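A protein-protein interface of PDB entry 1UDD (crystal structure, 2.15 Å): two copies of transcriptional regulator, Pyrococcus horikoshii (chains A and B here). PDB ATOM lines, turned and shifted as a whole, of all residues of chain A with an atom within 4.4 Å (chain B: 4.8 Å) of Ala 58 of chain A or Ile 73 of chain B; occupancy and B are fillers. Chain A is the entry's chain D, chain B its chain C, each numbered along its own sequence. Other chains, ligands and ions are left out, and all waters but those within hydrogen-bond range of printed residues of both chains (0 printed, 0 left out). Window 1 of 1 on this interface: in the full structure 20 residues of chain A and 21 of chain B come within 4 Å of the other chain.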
ATOM      1  N   THR A  54      22.818  26.298  -1.594  1.00  0.00           N
ATOM      2  CA  THR A  54      23.002  26.138  -3.020  1.00  0.00           C
ATOM      3  C   THR A  54      21.889  25.271  -3.616  1.00  0.00           C
ATOM      4  O   THR A  54      21.340  25.610  -4.665  1.00  0.00           O
ATOM      5  CB  THR A  54      24.390  25.505  -3.321  1.00  0.00           C
ATOM      6  OG1 THR A  54      25.433  26.332  -2.778  1.00  0.00           O
ATOM      7  CG2 THR A  54      24.594  25.370  -4.801  1.00  0.00           C
ATOM      8  N   ARG A  55      21.547  24.163  -2.954  1.00  0.00           N
ATOM      9  CA  ARG A  55      20.472  23.294  -3.447  1.00  0.00           C
ATOM     10  C   ARG A  55      19.156  24.040  -3.579  1.00  0.00           C
ATOM     11  O   ARG A  55      18.502  23.954  -4.621  1.00  0.00           O
ATOM     12  CB  ARG A  55      20.224  22.100  -2.523  1.00  0.00           C
ATOM     13  CG  ARG A  55      21.361  21.111  -2.437  1.00  0.00           C
ATOM     14  CD  ARG A  55      20.957  19.871  -1.628  1.00  0.00           C
ATOM     15  NE  ARG A  55      22.106  18.990  -1.421  1.00  0.00           N
ATOM     16  CZ  ARG A  55      22.719  18.328  -2.392  1.00  0.00           C
ATOM     17  NH1 ARG A  55      22.285  18.428  -3.647  1.00  0.00           N
ATOM     18  NH2 ARG A  55      23.794  17.598  -2.118  1.00  0.00           N
ATOM     19  N   ALA A  56      18.756  24.755  -2.523  1.00  0.00           N
ATOM     20  CA  ALA A  56      17.493  25.492  -2.555  1.00  0.00           C
ATOM     21  C   ALA A  56      17.494  26.550  -3.653  1.00  0.00           C
ATOM     22  O   ALA A  56      16.500  26.723  -4.342  1.00  0.00           O
ATOM     23  CB  ALA A  56      17.212  26.149  -1.200  1.00  0.00           C
ATOM     24  N   LEU A  57      18.607  27.264  -3.807  1.00  0.00           N
ATOM     25  CA  LEU A  57      18.690  28.300  -4.835  1.00  0.00           C
ATOM     26  C   LEU A  57      18.579  27.675  -6.230  1.00  0.00           C
ATOM     27  O   LEU A  57      17.981  28.265  -7.135  1.00  0.00           O
ATOM     28  CB  LEU A  57      19.998  29.085  -4.693  1.00  0.00           C
ATOM     29  CG  LEU A  57      20.008  30.155  -3.591  1.00  0.00           C
ATOM     30  CD1 LEU A  57      21.442  30.587  -3.280  1.00  0.00           C
ATOM     31  CD2 LEU A  57      19.170  31.355  -4.051  1.00  0.00           C
ATOM     32  N   ALA A  58      19.126  26.472  -6.397  1.00  0.00           N
ATOM     33  CA  ALA A  58      19.061  25.794  -7.700  1.00  0.00           C
ATOM     34  C   ALA A  58      17.606  25.471  -8.014  1.00  0.00           C
ATOM     35  O   ALA A  58      17.138  25.688  -9.132  1.00  0.00           O
ATOM     36  CB  ALA A  58      19.899  24.531  -7.689  1.00  0.00           C
ATOM     37  N   VAL A  59      16.873  24.990  -7.018  1.00  0.00           N
ATOM     38  CA  VAL A  59      15.461  24.689  -7.230  1.00  0.00           C
ATOM     39  C   VAL A  59      14.703  25.979  -7.557  1.00  0.00           C
ATOM     40  O   VAL A  59      13.962  26.039  -8.549  1.00  0.00           O
ATOM     41  CB  VAL A  59      14.874  23.967  -5.987  1.00  0.00           C
ATOM     42  CG1 VAL A  59      13.318  23.855  -6.078  1.00  0.00           C
ATOM     43  CG2 VAL A  59      15.502  22.571  -5.893  1.00  0.00           C
ATOM     44  N   ILE A  60      14.893  27.035  -6.770  1.00  0.00           N
ATOM     45  CA  ILE A  60      14.172  28.275  -7.072  1.00  0.00           C
ATOM     46  C   ILE A  60      14.452  28.747  -8.496  1.00  0.00           C
ATOM     47  O   ILE A  60      13.524  29.085  -9.246  1.00  0.00           O
ATOM     48  CB  ILE A  60      14.520  29.429  -6.085  1.00  0.00           C
ATOM     49  CG1 ILE A  60      14.183  29.032  -4.645  1.00  0.00           C
ATOM     50  CG2 ILE A  60      13.697  30.658  -6.426  1.00  0.00           C
ATOM     51  CD1 ILE A  60      14.695  30.022  -3.599  1.00  0.00           C
ATOM     52  N   SER A  61      15.721  28.756  -8.894  1.00  0.00           N
ATOM     53  CA  SER A  61      16.063  29.203 -10.247  1.00  0.00           C
ATOM     54  C   SER A  61      15.470  28.293 -11.338  1.00  0.00           C
ATOM     55  O   SER A  61      15.071  28.770 -12.407  1.00  0.00           O
ATOM     56  CB  SER A  61      17.584  29.277 -10.409  1.00  0.00           C
ATOM     57  OG  SER A  61      18.131  27.978 -10.407  1.00  0.00           O
ATOM     58  N   SER A  62      15.408  26.989 -11.064  1.00  0.00           N
ATOM     59  CA  SER A  62      14.845  26.027 -12.023  1.00  0.00           C
ATOM     60  C   SER A  62      13.391  26.382 -12.334  1.00  0.00           C
ATOM     61  O   SER A  62      12.860  26.020 -13.387  1.00  0.00           O
ATOM     62  CB  SER A  62      14.879  24.608 -11.440  1.00  0.00           C
ATOM     63  OG  SER A  62      13.756  24.386 -10.576  1.00  0.00           O
ATOM     64  N   ALA A  76      23.749  30.907  -6.677  1.00  0.00           N
ATOM     65  CA  ALA A  76      23.932  29.510  -6.284  1.00  0.00           C
ATOM     66  C   ALA A  76      25.349  29.080  -6.644  1.00  0.00           C
ATOM     67  O   ALA A  76      26.036  28.404  -5.874  1.00  0.00           O
ATOM     68  CB  ALA A  76      22.906  28.625  -7.013  1.00  0.00           C
ATOM     69  N   ARG A  77      25.776  29.498  -7.826  1.00  0.00           N
ATOM     70  CA  ARG A  77      27.099  29.180  -8.321  1.00  0.00           C
ATOM     71  C   ARG A  77      28.157  29.798  -7.413  1.00  0.00           C
ATOM     72  O   ARG A  77      29.146  29.149  -7.054  1.00  0.00           O
ATOM     73  CB  ARG A  77      27.230  29.697  -9.755  1.00  0.00           C
ATOM     74  CG  ARG A  77      28.592  29.529 -10.375  1.00  0.00           C
ATOM     75  CD  ARG A  77      29.450  30.736 -10.090  1.00  0.00           C
ATOM     76  NE  ARG A  77      30.645  30.739 -10.915  1.00  0.00           N
ATOM     77  CZ  ARG A  77      31.508  31.748 -10.969  1.00  0.00           C
ATOM     78  NH1 ARG A  77      31.302  32.838 -10.242  1.00  0.00           N
ATOM     79  NH2 ARG A  77      32.578  31.667 -11.748  1.00  0.00           N
ATOM     80  N   VAL A  80      28.864  27.736  -4.032  1.00  0.00           N
ATOM     81  CA  VAL A  80      29.709  26.548  -4.115  1.00  0.00           C
ATOM     82  C   VAL A  80      31.017  26.745  -4.852  1.00  0.00           C
ATOM     83  O   VAL A  80      31.773  25.796  -5.043  1.00  0.00           O
ATOM     84  CB  VAL A  80      28.951  25.367  -4.759  1.00  0.00           C
ATOM     85  CG1 VAL A  80      27.902  24.868  -3.808  1.00  0.00           C
ATOM     86  CG2 VAL A  80      28.315  25.798  -6.081  1.00  0.00           C
ATOM     87  N   ALA B  58      19.945  22.821 -13.465  1.00  0.00           N
ATOM     88  CA  ALA B  58      19.702  23.305 -12.108  1.00  0.00           C
ATOM     89  C   ALA B  58      19.073  22.179 -11.264  1.00  0.00           C
ATOM     90  O   ALA B  58      19.500  21.923 -10.141  1.00  0.00           O
ATOM     91  CB  ALA B  58      18.773  24.517 -12.149  1.00  0.00           C
ATOM     92  N   SER B  61      21.571  19.467 -10.591  1.00  0.00           N
ATOM     93  CA  SER B  61      22.488  19.992  -9.576  1.00  0.00           C
ATOM     94  C   SER B  61      21.872  19.987  -8.176  1.00  0.00           C
ATOM     95  O   SER B  61      22.528  19.646  -7.192  1.00  0.00           O
ATOM     96  CB  SER B  61      22.893  21.424  -9.930  1.00  0.00           C
ATOM     97  OG  SER B  61      23.330  22.091  -8.756  1.00  0.00           O
ATOM     98  N   SER B  62      20.601  20.358  -8.084  1.00  0.00           N
ATOM     99  CA  SER B  62      19.940  20.386  -6.780  1.00  0.00           C
ATOM    100  C   SER B  62      19.900  19.026  -6.064  1.00  0.00           C
ATOM    101  O   SER B  62      19.770  18.963  -4.846  1.00  0.00           O
ATOM    102  CB  SER B  62      18.511  20.901  -6.925  1.00  0.00           C
ATOM    103  OG  SER B  62      17.693  19.956  -7.605  1.00  0.00           O
ATOM    104  N   MET B  69      27.724  18.499  -7.739  1.00  0.00           N
ATOM    105  CA  MET B  69      26.716  19.546  -7.732  1.00  0.00           C
ATOM    106  C   MET B  69      27.328  20.893  -8.135  1.00  0.00           C
ATOM    107  O   MET B  69      26.714  21.668  -8.861  1.00  0.00           O
ATOM    108  CB  MET B  69      26.104  19.675  -6.335  1.00  0.00           C
ATOM    109  CG  MET B  69      25.211  20.878  -6.190  1.00  0.00           C
ATOM    110  SD  MET B  69      25.374  21.648  -4.565  1.00  0.00           S
ATOM    111  CE  MET B  69      24.354  20.566  -3.617  1.00  0.00           C
ATOM    112  N   ALA B  70      28.532  21.174  -7.651  1.00  0.00           N
ATOM    113  CA  ALA B  70      29.189  22.436  -7.971  1.00  0.00           C
ATOM    114  C   ALA B  70      29.578  22.470  -9.443  1.00  0.00           C
ATOM    115  O   ALA B  70      29.436  23.498 -10.106  1.00  0.00           O
ATOM    116  CB  ALA B  70      30.430  22.632  -7.095  1.00  0.00           C
ATOM    117  N   GLU B  71      30.074  21.340  -9.938  1.00  0.00           N
ATOM    118  CA  GLU B  71      30.478  21.199 -11.337  1.00  0.00           C
ATOM    119  C   GLU B  71      29.257  21.453 -12.221  1.00  0.00           C
ATOM    120  O   GLU B  71      29.348  22.111 -13.256  1.00  0.00           O
ATOM    121  CB  GLU B  71      31.017  19.779 -11.580  1.00  0.00           C
ATOM    122  CG  GLU B  71      31.761  19.579 -12.894  1.00  0.00           C
ATOM    123  CD  GLU B  71      32.269  18.143 -13.092  1.00  0.00           C
ATOM    124  OE1 GLU B  71      32.738  17.522 -12.112  1.00  0.00           O
ATOM    125  OE2 GLU B  71      32.211  17.642 -14.237  1.00  0.00           O
ATOM    126  N   LEU B  72      28.104  20.951 -11.792  1.00  0.00           N
ATOM    127  CA  LEU B  72      26.871  21.117 -12.565  1.00  0.00           C
ATOM    128  C   LEU B  72      26.244  22.502 -12.506  1.00  0.00           C
ATOM    129  O   LEU B  72      25.733  22.991 -13.525  1.00  0.00           O
ATOM    130  CB  LEU B  72      25.840  20.057 -12.152  1.00  0.00           C
ATOM    131  CG  LEU B  72      25.738  18.817 -13.048  1.00  0.00           C
ATOM    132  CD1 LEU B  72      27.037  18.582 -13.805  1.00  0.00           C
ATOM    133  CD2 LEU B  72      25.377  17.606 -12.194  1.00  0.00           C
ATOM    134  N   ILE B  73      26.263  23.145 -11.337  1.00  0.00           N
ATOM    135  CA  ILE B  73      25.679  24.478 -11.244  1.00  0.00           C
ATOM    136  C   ILE B  73      26.554  25.465 -12.053  1.00  0.00           C
ATOM    137  O   ILE B  73      26.052  26.454 -12.593  1.00  0.00           O
ATOM    138  CB  ILE B  73      25.525  24.931  -9.764  1.00  0.00           C
ATOM    139  CG1 ILE B  73      24.430  25.992  -9.648  1.00  0.00           C
ATOM    140  CG2 ILE B  73      26.806  25.553  -9.249  1.00  0.00           C
ATOM    141  CD1 ILE B  73      23.009  25.483  -9.943  1.00  0.00           C
ATOM    142  N   GLU B  74      27.851  25.182 -12.150  1.00  0.00           N
ATOM    143  CA  GLU B  74      28.781  26.029 -12.911  1.00  0.00           C
ATOM    144  C   GLU B  74      28.406  25.997 -14.386  1.00  0.00           C
ATOM    145  O   GLU B  74      28.422  27.026 -15.080  1.00  0.00           O
ATOM    146  CB  GLU B  74      30.213  25.519 -12.770  1.00  0.00           C
ATOM    147  CG  GLU B  74      31.238  26.236 -13.671  1.00  0.00           C
ATOM    148  CD  GLU B  74      31.481  27.687 -13.249  1.00  0.00           C
ATOM    149  OE1 GLU B  74      31.708  27.926 -12.047  1.00  0.00           O
ATOM    150  OE2 GLU B  74      31.450  28.593 -14.117  1.00  0.00           O
ATOM    151  N   LEU B  75      28.069  24.799 -14.853  1.00  0.00           N
ATOM    152  CA  LEU B  75      27.669  24.585 -16.235  1.00  0.00           C
ATOM    153  C   LEU B  75      26.320  25.279 -16.486  1.00  0.00           C
ATOM    154  O   LEU B  75      26.104  25.873 -17.548  1.00  0.00           O
ATOM    155  CB  LEU B  75      27.553  23.085 -16.499  1.00  0.00           C
ATOM    156  CG  LEU B  75      27.480  22.551 -17.931  1.00  0.00           C
ATOM    157  CD1 LEU B  75      28.757  22.929 -18.675  1.00  0.00           C
ATOM    158  CD2 LEU B  75      27.321  21.025 -17.897  1.00  0.00           C
ATOM    159  N   ALA B  76      25.416  25.202 -15.508  1.00  0.00           N
ATOM    160  CA  ALA B  76      24.109  25.837 -15.633  1.00  0.00           C
ATOM    161  C   ALA B  76      24.320  27.350 -15.688  1.00  0.00           C
ATOM    162  O   ALA B  76      23.703  28.041 -16.495  1.00  0.00           O
ATOM    163  CB  ALA B  76      23.227  25.474 -14.439  1.00  0.00           C
ATOM    164  N   ARG B  77      25.201  27.839 -14.819  1.00  0.00           N
ATOM    165  CA  ARG B  77      25.528  29.258 -14.723  1.00  0.00           C
ATOM    166  C   ARG B  77      26.118  29.777 -16.040  1.00  0.00           C
ATOM    167  O   ARG B  77      25.715  30.825 -16.536  1.00  0.00           O
ATOM    168  CB  ARG B  77      26.507  29.474 -13.561  1.00  0.00           C
ATOM    169  CG  ARG B  77      26.954  30.913 -13.347  1.00  0.00           C
ATOM    170  CD  ARG B  77      28.252  31.188 -14.078  1.00  0.00           C
ATOM    171  NE  ARG B  77      28.791  32.497 -13.732  1.00  0.00           N
ATOM    172  CZ  ARG B  77      29.983  32.942 -14.119  1.00  0.00           C
ATOM    173  NH1 ARG B  77      30.773  32.185 -14.871  1.00  0.00           N
ATOM    174  NH2 ARG B  77      30.383  34.151 -13.751  1.00  0.00           N
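The backbone carbonyl oxygen of Ser 62 of chain B lies within hydrogen-bond range of the guanidinium group of Arg 55 of chain A. The side-chain carboxylate (OE1) of Glu 74 of chain B is in salt-bridge range of the guanidinium group (NE) of Arg 77 of chain A, at 3.2 Å.
The side-chain hydroxyl (OG) of Ser 61 of chain B lies close to the backbone carbonyl oxygen (O) of Met 69 of chain B (3.4 Å). The guanidinium group (NH1) of Arg 77 of chain B lies within salt-bridge range of the side-chain carboxylate (OE2) of Glu 74 of chain B, 3.7 Å away. The backbone carbonyl oxygen (O) of Leu 57 of chain A sits at hydrogen-bond distance from the side-chain hydroxyl (OG) of Ser 61 of chain A (3.3 Å). OG of Ser 61 of chain A sits at hydrogen-bond distance from O of Ala 58 of chain A. The side-chain hydroxyl (OG) of Ser 62 of chain A sits at hydrogen-bond distance from the backbone carbonyl oxygen (O) of Val 59 of chain A (2.6 Å).
Among the printed residues, pairs that only touch across the chains: Arg 55 of chain A with Met 69 of chain B, Val 80 of chain A with Ile 73 of chain B, Val 59 of chain A with Ser 62 of chain B, Ala 58 of chain A with Ala 58 of chain B, Arg 77 of chain A with Arg 77 of chain B, Arg 77 of chain A with Ile 73 of chain B, Arg 55 of chain A with Ser 61 of chain B, Thr 54 of chain A with Met 69 of chain B, Val 80 of chain A with Ala 70 of chain B, Ser 61 of chain A with Ala 58 of chain B, Ala 58 of chain A with Ile 73 of chain B, Ser 62 of chain A with Ala 58 of chain B and Ala 58 of chain A with Ser 62 of chain B.
Ala 58 of chain A touches three residues of chain B. Printed residues of chain B within 4 Å of Ser 61 of chain A: Ala 58. Ala 76 of chain A touches none of the printed residues of chain B. Of the printed residues of chain B, Val 80 of chain A touches Ala 70 and Ile 73. Of the printed residues of chain A, Ser 61 of chain B touches Arg 55 (3.8 Å). Ile 73 of chain B touches three residues of chain A. The nearest residue of chain B that does not touch Ala 58 of chain A is Ser 61 of chain B (4.3 Å). The nearest residue of chain A that does not touch Ile 73 of chain B is Ala 76 of chain A (4.02 Å). The nearest printed residue of chain B that does not touch Arg 55 of chain A is Ala 58 of chain B (6.0 Å).
Printed residues of chain B that touch a printed residue of chain A: Ala 58, Ser 61, Ser 62, Met 69, Ala 70, Ile 73, Glu 74 and Arg 77. Hydrophobic or aromatic side chains of chain B within 4 Å of the printed part of chain A: Ala 58, Met 69, Ala 70 and Ile 73. Along chain B the printed residues that touch a printed residue of chain A span positions 58 to 77. Among the printed residues, 15 pairs touch across the chains.
Ala 58 of chain A touches its own counterpart, Ala 58 of chain B. Ala 58 of chain A touches Ser 62 of chain B, and with the chains exchanged Ser 62 of chain A touches Ala 58 of chain B. Ser 61 of chain A touches Ala 58 of chain B, but with the chains exchanged Ala 58 of chain A does not touch Ser 61 of chain B (4.3 Å). Arg 77 of chain B touches its own counterpart, Arg 77 of chain A. 5 positions are printed for both chains. Of the 15 pairs that touch across the chains among the printed residues, 4 have their exchanged pair printed and touching as well.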
